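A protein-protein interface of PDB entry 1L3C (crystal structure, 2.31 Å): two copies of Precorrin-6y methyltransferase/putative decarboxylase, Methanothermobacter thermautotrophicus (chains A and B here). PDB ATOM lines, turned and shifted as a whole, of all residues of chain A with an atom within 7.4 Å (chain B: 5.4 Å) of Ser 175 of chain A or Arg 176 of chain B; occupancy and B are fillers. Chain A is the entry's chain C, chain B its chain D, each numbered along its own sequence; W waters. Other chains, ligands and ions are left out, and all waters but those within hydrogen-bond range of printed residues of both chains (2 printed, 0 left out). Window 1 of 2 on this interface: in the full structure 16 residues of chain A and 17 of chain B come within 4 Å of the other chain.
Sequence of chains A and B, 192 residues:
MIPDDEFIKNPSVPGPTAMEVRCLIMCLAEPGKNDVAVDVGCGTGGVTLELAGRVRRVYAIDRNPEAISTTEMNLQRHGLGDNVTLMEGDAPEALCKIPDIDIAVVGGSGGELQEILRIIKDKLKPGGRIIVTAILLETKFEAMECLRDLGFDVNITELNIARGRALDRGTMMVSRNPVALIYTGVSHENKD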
ATOM      1  N   ASN A 160       1.812  -0.874 -33.002  1.00  0.00           N
ATOM      2  CA  ASN A 160       1.793  -0.606 -31.584  1.00  0.00           C
ATOM      3  C   ASN A 160       0.916  -1.697 -31.055  1.00  0.00           C
ATOM      4  O   ASN A 160      -0.283  -1.763 -31.378  1.00  0.00           O
ATOM      5  CB  ASN A 160       1.195   0.744 -31.311  1.00  0.00           C
ATOM      6  CG  ASN A 160       2.232   1.807 -31.290  1.00  0.00           C
ATOM      7  OD1 ASN A 160       2.897   1.994 -30.270  1.00  0.00           O
ATOM      8  ND2 ASN A 160       2.436   2.478 -32.428  1.00  0.00           N
ATOM      9  N   ILE A 161       1.533  -2.587 -30.292  1.00  0.00           N
ATOM     10  CA  ILE A 161       0.843  -3.747 -29.745  1.00  0.00           C
ATOM     11  C   ILE A 161       0.757  -3.717 -28.231  1.00  0.00           C
ATOM     12  O   ILE A 161       1.720  -3.374 -27.570  1.00  0.00           O
ATOM     13  CB  ILE A 161       1.621  -5.013 -30.115  1.00  0.00           C
ATOM     14  CG1 ILE A 161       1.896  -5.025 -31.618  1.00  0.00           C
ATOM     15  CG2 ILE A 161       0.868  -6.261 -29.714  1.00  0.00           C
ATOM     16  CD1 ILE A 161       3.159  -5.785 -31.957  1.00  0.00           C
ATOM     17  N   ALA A 162      -0.387  -4.110 -27.694  1.00  0.00           N
ATOM     18  CA  ALA A 162      -0.582  -4.182 -26.264  1.00  0.00           C
ATOM     19  C   ALA A 162      -1.171  -5.567 -26.045  1.00  0.00           C
ATOM     20  O   ALA A 162      -1.996  -6.036 -26.827  1.00  0.00           O
ATOM     21  CB  ALA A 162      -1.549  -3.108 -25.803  1.00  0.00           C
ATOM     22  N   ARG A 163      -0.691  -6.251 -25.020  1.00  0.00           N
ATOM     23  CA  ARG A 163      -1.174  -7.578 -24.681  1.00  0.00           C
ATOM     24  C   ARG A 163      -1.712  -7.505 -23.282  1.00  0.00           C
ATOM     25  O   ARG A 163      -1.236  -6.712 -22.484  1.00  0.00           O
ATOM     26  CB  ARG A 163      -0.038  -8.581 -24.707  1.00  0.00           C
ATOM     27  CG  ARG A 163       0.626  -8.766 -26.059  1.00  0.00           C
ATOM     28  CD  ARG A 163       1.764  -9.745 -25.927  1.00  0.00           C
ATOM     29  NE  ARG A 163       2.561  -9.807 -27.136  1.00  0.00           N
ATOM     30  CZ  ARG A 163       3.860 -10.080 -27.149  1.00  0.00           C
ATOM     31  NH1 ARG A 163       4.495 -10.311 -26.010  1.00  0.00           N
ATOM     32  NH2 ARG A 163       4.511 -10.142 -28.307  1.00  0.00           N
ATOM     33  N   MET A 172      -4.536  -5.938 -17.118  1.00  0.00           N
ATOM     34  CA  MET A 172      -3.948  -4.669 -17.504  1.00  0.00           C
ATOM     35  C   MET A 172      -3.239  -4.812 -18.857  1.00  0.00           C
ATOM     36  O   MET A 172      -2.635  -5.851 -19.146  1.00  0.00           O
ATOM     37  CB  MET A 172      -2.984  -4.158 -16.457  1.00  0.00           C
ATOM     38  CG  MET A 172      -1.648  -4.804 -16.518  1.00  0.00           C
ATOM     39  SD  MET A 172      -0.319  -3.668 -15.679  1.00  0.00           S
ATOM     40  CE  MET A 172       0.681  -5.006 -14.744  1.00  0.00           C
ATOM     41  N   MET A 173      -3.358  -3.787 -19.696  1.00  0.00           N
ATOM     42  CA  MET A 173      -2.753  -3.820 -21.021  1.00  0.00           C
ATOM     43  C   MET A 173      -1.298  -3.402 -20.920  1.00  0.00           C
ATOM     44  O   MET A 173      -0.981  -2.359 -20.352  1.00  0.00           O
ATOM     45  CB  MET A 173      -3.524  -2.905 -21.991  1.00  0.00           C
ATOM     46  CG  MET A 173      -4.997  -3.275 -22.137  1.00  0.00           C
ATOM     47  SD  MET A 173      -5.192  -5.180 -22.571  1.00  0.00           S
ATOM     48  CE  MET A 173      -4.703  -5.120 -24.502  1.00  0.00           C
ATOM     49  N   VAL A 174      -0.410  -4.231 -21.445  1.00  0.00           N
ATOM     50  CA  VAL A 174       1.011  -3.945 -21.404  1.00  0.00           C
ATOM     51  C   VAL A 174       1.541  -3.720 -22.804  1.00  0.00           C
ATOM     52  O   VAL A 174       1.426  -4.569 -23.670  1.00  0.00           O
ATOM     53  CB  VAL A 174       1.803  -5.086 -20.725  1.00  0.00           C
ATOM     54  CG1 VAL A 174       3.289  -4.792 -20.737  1.00  0.00           C
ATOM     55  CG2 VAL A 174       1.361  -5.228 -19.292  1.00  0.00           C
ATOM     56  N   SER A 175       2.181  -2.579 -22.997  1.00  0.00           N
ATOM     57  CA  SER A 175       2.740  -2.198 -24.287  1.00  0.00           C
ATOM     58  C   SER A 175       4.091  -2.740 -24.659  1.00  0.00           C
ATOM     59  O   SER A 175       4.920  -3.055 -23.819  1.00  0.00           O
ATOM     60  CB  SER A 175       2.782  -0.689 -24.445  1.00  0.00           C
ATOM     61  OG  SER A 175       1.481  -0.190 -24.722  1.00  0.00           O
ATOM     62  N   ARG A 176       4.265  -2.882 -25.963  1.00  0.00           N
ATOM     63  CA  ARG A 176       5.484  -3.332 -26.588  1.00  0.00           C
ATOM     64  C   ARG A 176       5.979  -2.068 -27.270  1.00  0.00           C
ATOM     65  O   ARG A 176       5.163  -1.236 -27.674  1.00  0.00           O
ATOM     66  CB  ARG A 176       5.146  -4.360 -27.666  1.00  0.00           C
ATOM     67  CG  ARG A 176       4.639  -5.651 -27.130  1.00  0.00           C
ATOM     68  CD  ARG A 176       5.759  -6.264 -26.376  1.00  0.00           C
ATOM     69  NE  ARG A 176       5.279  -7.279 -25.469  1.00  0.00           N
ATOM     70  CZ  ARG A 176       6.054  -7.883 -24.575  1.00  0.00           C
ATOM     71  NH1 ARG A 176       7.337  -7.581 -24.465  1.00  0.00           N
ATOM     72  NH2 ARG A 176       5.534  -8.825 -23.801  1.00  0.00           N
ATOM     73  N   ASN A 177       7.288  -1.889 -27.376  1.00  0.00           N
ATOM     74  CA  ASN A 177       7.800  -0.709 -28.056  1.00  0.00           C
ATOM     75  C   ASN A 177       7.354  -0.720 -29.502  1.00  0.00           C
ATOM     76  O   ASN A 177       7.230  -1.775 -30.109  1.00  0.00           O
ATOM     77  CB  ASN A 177       9.305  -0.663 -27.984  1.00  0.00           C
ATOM     78  CG  ASN A 177       9.790  -0.429 -26.588  1.00  0.00           C
ATOM     79  OD1 ASN A 177       9.041   0.038 -25.732  1.00  0.00           O
ATOM     80  ND2 ASN A 177      11.041  -0.760 -26.334  1.00  0.00           N
ATOM     81  N   PRO A 178       7.087   0.449 -30.074  1.00  0.00           N
ATOM     82  CA  PRO A 178       6.647   0.504 -31.474  1.00  0.00           C
ATOM     83  C   PRO A 178       7.696  -0.087 -32.418  1.00  0.00           C
ATOM     84  O   PRO A 178       8.902   0.096 -32.237  1.00  0.00           O
ATOM     85  CB  PRO A 178       6.507   2.005 -31.744  1.00  0.00           C
ATOM     86  CG  PRO A 178       6.455   2.630 -30.362  1.00  0.00           C
ATOM     87  CD  PRO A 178       7.363   1.794 -29.546  1.00  0.00           C
ATOM     88  N   ASP B   4       8.834  13.116 -15.103  1.00  0.00           N
ATOM     89  CA  ASP B   4       8.871  11.865 -14.354  1.00  0.00           C
ATOM     90  C   ASP B   4      10.152  11.604 -13.567  1.00  0.00           C
ATOM     91  O   ASP B   4      10.115  11.020 -12.486  1.00  0.00           O
ATOM     92  CB  ASP B   4       8.645  10.674 -15.289  1.00  0.00           C
ATOM     93  CG  ASP B   4       7.342  10.757 -16.048  1.00  0.00           C
ATOM     94  OD1 ASP B   4       6.665  11.813 -15.995  1.00  0.00           O
ATOM     95  OD2 ASP B   4       7.001   9.753 -16.705  1.00  0.00           O
ATOM     96  N   ALA B  18       2.678   9.146 -16.080  1.00  0.00           N
ATOM     97  CA  ALA B  18       3.488   9.724 -17.147  1.00  0.00           C
ATOM     98  C   ALA B  18       3.105  11.180 -17.309  1.00  0.00           C
ATOM     99  O   ALA B  18       1.916  11.519 -17.289  1.00  0.00           O
ATOM    100  CB  ALA B  18       3.268   8.978 -18.468  1.00  0.00           C
ATOM    101  N   ASN B 160      -1.274   6.382 -26.010  1.00  0.00           N
ATOM    102  CA  ASN B 160      -0.168   5.481 -26.213  1.00  0.00           C
ATOM    103  C   ASN B 160       0.966   6.437 -26.506  1.00  0.00           C
ATOM    104  O   ASN B 160       0.940   7.168 -27.503  1.00  0.00           O
ATOM    105  CB  ASN B 160      -0.442   4.557 -27.372  1.00  0.00           C
ATOM    106  CG  ASN B 160      -1.093   3.291 -26.931  1.00  0.00           C
ATOM    107  OD1 ASN B 160      -0.426   2.368 -26.466  1.00  0.00           O
ATOM    108  ND2 ASN B 160      -2.407   3.236 -27.041  1.00  0.00           N
ATOM    109  N   ILE B 161       1.931   6.461 -25.596  1.00  0.00           N
ATOM    110  CA  ILE B 161       3.045   7.370 -25.686  1.00  0.00           C
ATOM    111  C   ILE B 161       4.345   6.641 -25.862  1.00  0.00           C
ATOM    112  O   ILE B 161       4.562   5.608 -25.227  1.00  0.00           O
ATOM    113  CB  ILE B 161       3.153   8.182 -24.372  1.00  0.00           C
ATOM    114  CG1 ILE B 161       1.807   8.810 -24.025  1.00  0.00           C
ATOM    115  CG2 ILE B 161       4.199   9.277 -24.489  1.00  0.00           C
ATOM    116  CD1 ILE B 161       1.622   8.972 -22.547  1.00  0.00           C
ATOM    117  N   ALA B 162       5.202   7.191 -26.720  1.00  0.00           N
ATOM    118  CA  ALA B 162       6.537   6.657 -26.956  1.00  0.00           C
ATOM    119  C   ALA B 162       7.494   7.852 -26.841  1.00  0.00           C
ATOM    120  O   ALA B 162       7.206   8.935 -27.345  1.00  0.00           O
ATOM    121  CB  ALA B 162       6.637   6.021 -28.326  1.00  0.00           C
ATOM    122  N   ARG B 163       8.572   7.672 -26.095  1.00  0.00           N
ATOM    123  CA  ARG B 163       9.563   8.703 -25.914  1.00  0.00           C
ATOM    124  C   ARG B 163      10.854   8.184 -26.504  1.00  0.00           C
ATOM    125  O   ARG B 163      11.132   6.980 -26.444  1.00  0.00           O
ATOM    126  CB  ARG B 163       9.775   8.960 -24.426  1.00  0.00           C
ATOM    127  CG  ARG B 163       8.539   9.406 -23.691  1.00  0.00           C
ATOM    128  CD  ARG B 163       8.884   9.672 -22.264  1.00  0.00           C
ATOM    129  NE  ARG B 163       7.708   9.982 -21.463  1.00  0.00           N
ATOM    130  CZ  ARG B 163       7.580   9.661 -20.175  1.00  0.00           C
ATOM    131  NH1 ARG B 163       8.556   9.015 -19.537  1.00  0.00           N
ATOM    132  NH2 ARG B 163       6.484  10.003 -19.514  1.00  0.00           N
ATOM    133  N   VAL B 174      10.710   4.253 -27.010  1.00  0.00           N
ATOM    134  CA  VAL B 174      10.347   3.399 -25.901  1.00  0.00           C
ATOM    135  C   VAL B 174       8.935   3.713 -25.458  1.00  0.00           C
ATOM    136  O   VAL B 174       8.597   4.846 -25.149  1.00  0.00           O
ATOM    137  CB  VAL B 174      11.326   3.559 -24.704  1.00  0.00           C
ATOM    138  CG1 VAL B 174      10.872   2.711 -23.537  1.00  0.00           C
ATOM    139  CG2 VAL B 174      12.741   3.147 -25.119  1.00  0.00           C
ATOM    140  N   SER B 175       8.123   2.678 -25.414  1.00  0.00           N
ATOM    141  CA  SER B 175       6.734   2.783 -25.040  1.00  0.00           C
ATOM    142  C   SER B 175       6.427   2.785 -23.570  1.00  0.00           C
ATOM    143  O   SER B 175       7.160   2.220 -22.748  1.00  0.00           O
ATOM    144  CB  SER B 175       5.938   1.658 -25.679  1.00  0.00           C
ATOM    145  OG  SER B 175       5.719   1.960 -27.050  1.00  0.00           O
ATOM    146  N   ARG B 176       5.315   3.444 -23.265  1.00  0.00           N
ATOM    147  CA  ARG B 176       4.746   3.550 -21.927  1.00  0.00           C
ATOM    148  C   ARG B 176       3.485   2.698 -22.060  1.00  0.00           C
ATOM    149  O   ARG B 176       2.940   2.583 -23.166  1.00  0.00           O
ATOM    150  CB  ARG B 176       4.342   4.996 -21.666  1.00  0.00           C
ATOM    151  CG  ARG B 176       5.491   5.918 -21.562  1.00  0.00           C
ATOM    152  CD  ARG B 176       6.229   5.521 -20.359  1.00  0.00           C
ATOM    153  NE  ARG B 176       7.583   6.045 -20.366  1.00  0.00           N
ATOM    154  CZ  ARG B 176       8.479   5.787 -19.418  1.00  0.00           C
ATOM    155  NH1 ARG B 176       8.149   5.020 -18.382  1.00  0.00           N
ATOM    156  NH2 ARG B 176       9.695   6.316 -19.479  1.00  0.00           N
ATOM    157  N   ASN B 177       3.056   2.032 -20.991  1.00  0.00           N
ATOM    158  CA  ASN B 177       1.835   1.230 -21.070  1.00  0.00           C
ATOM    159  C   ASN B 177       0.685   2.157 -21.355  1.00  0.00           C
ATOM    160  O   ASN B 177       0.675   3.277 -20.878  1.00  0.00           O
ATOM    161  CB  ASN B 177       1.584   0.510 -19.768  1.00  0.00           C
ATOM    162  CG  ASN B 177       2.573  -0.599 -19.549  1.00  0.00           C
ATOM    163  OD1 ASN B 177       3.203  -1.076 -20.504  1.00  0.00           O
ATOM    164  ND2 ASN B 177       2.738  -1.014 -18.301  1.00  0.00           N
ATOM    165  N   PRO B 178      -0.303   1.716 -22.151  1.00  0.00           N
ATOM    166  CA  PRO B 178      -1.473   2.546 -22.502  1.00  0.00           C
ATOM    167  C   PRO B 178      -2.234   2.968 -21.264  1.00  0.00           C
ATOM    168  O   PRO B 178      -2.380   2.182 -20.320  1.00  0.00           O
ATOM    169  CB  PRO B 178      -2.350   1.609 -23.328  1.00  0.00           C
ATOM    170  CG  PRO B 178      -1.414   0.486 -23.748  1.00  0.00           C
ATOM    171  CD  PRO B 178      -0.476   0.328 -22.611  1.00  0.00           C
HETATM  172  O   HOH W   1       3.866   3.799 -28.573  1.00  0.00           O
HETATM  173  O   HOH W   2       5.549  -1.282 -21.901  1.00  0.00           O
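The side-chain hydroxyl of Ser 175 of chain A sits at hydrogen-bond distance from the backbone carbonyl oxygen of Arg 176 of chain B (3.5 Å). OD1 of Asn 177 of chain B sits at hydrogen-bond distance from N of Ser 175 of chain A (3.1 Å). OG of Ser 175 of chain B is in hydrogen-bond range of O of Arg 176 of chain A (3.3 Å). N of Ser 175 of chain B sits at hydrogen-bond distance from OD1 of Asn 177 of chain A, at 2.8 Å.
The backbone NH of Arg 176 of chain A sits at hydrogen-bond distance from the backbone carbonyl oxygen of Ile 161 of chain A (3.0 Å). The backbone NH (N) of Val 174 of chain A lies within hydrogen-bond range of the backbone carbonyl oxygen (O) of Arg 163 of chain A, 2.8 Å away. N of Arg 176 of chain B is in hydrogen-bond range of O of Ile 161 of chain B (3.0 Å). O of Arg 163 of chain B is in hydrogen-bond range of N of Val 174 of chain B (2.8 Å).
Asn 177 of chain B touches Met 173 of chain A. CD of Pro 178 of chain B touches O of Met 173 of chain A, at 3.5 Å. Asn 177 of chain B touches Val 174 of chain A. Ser 175 of chain A touches Asn 160 of chain B (OG to OD1, 3.6 Å). CD of Pro 178 of chain B touches OG of Ser 175 of chain A, at 2.9 Å. Asn 177 of chain A touches Val 174 of chain B (OD1 to CA, 3.6 Å). Ala 162 of chain B touches Pro 178 of chain A. Ser 175 of chain B touches Pro 178 of chain A.
Of chain B, only Asn 160, Arg 176, Asn 177 and Pro 178 come within 4 Å of Ser 175 of chain A. Arg 176 of chain B touches just one residue of chain A: Ser 175. Of the printed residues of chain A, Ser 175 of chain B touches Arg 176, Asn 177 and Pro 178. Of the printed residues of chain A, Asn 160 of chain B touches Ser 175. Printed residues of chain B within 4 Å of Met 173 of chain A: Asn 177 (3.9 Å) and Pro 178 (3.5 Å). Asn 160 of chain A touches none of the printed residues of chain B. The nearest residue of chain B that does not touch Ser 175 of chain A is Ser 175 of chain B (4.1 Å). The nearest residue of chain A that does not touch Arg 176 of chain B is Asn 177 of chain A (5.6 Å). The nearest printed residue of chain B that does not touch Met 173 of chain A is Arg 176 of chain B (6.9 Å).
Of the 11 printed residues of chain B, 7 touch a printed residue of chain A. Printed residues of chain B that touch a printed residue of chain A: Asn 160, Ala 162, Val 174, Ser 175, Arg 176, Asn 177 and Pro 178. Hydrophobic or aromatic side chains of chain B within 4 Å of the printed part of chain A: Ala 162, Val 174 and Pro 178. Of the 11 printed residues of chain A, 6 touch a printed residue of chain B. Printed residues of chain A that touch a printed residue of chain B: Met 173, Val 174, Ser 175, Arg 176, Asn 177 and Pro 178. Hydrophobic or aromatic side chains of chain A that line the printed part of chain B: Val 174 and Pro 178. Among the printed residues, 12 pairs touch across the chains.
Val 174 of chain A touches Asn 177 of chain B, and with the chains exchanged Asn 177 of chain A touches Val 174 of chain B. Ser 175 of chain A touches Asn 160 of chain B, but with the chains exchanged Asn 160 of chain A does not touch Ser 175 of chain B (4.3 Å). Ser 175 of chain A touches Arg 176 of chain B, and with the chains exchanged Arg 176 of chain A touches Ser 175 of chain B. Pro 178 of chain A touches Ala 162 of chain B, but with the chains exchanged Ala 162 of chain A does not touch Pro 178 of chain B (4.1 Å). Of the 12 pairs that touch across the chains among the printed residues, 8 have their exchanged pair printed and touching as well.
Water W1 bridges OD1 of Asn 160 of chain A and OG of Ser 175 of chain B. Water W2 bridges O of Ser 175 of chain A (2.7 Å) and OD1 of Asn 177 of chain B (2.7 Å).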
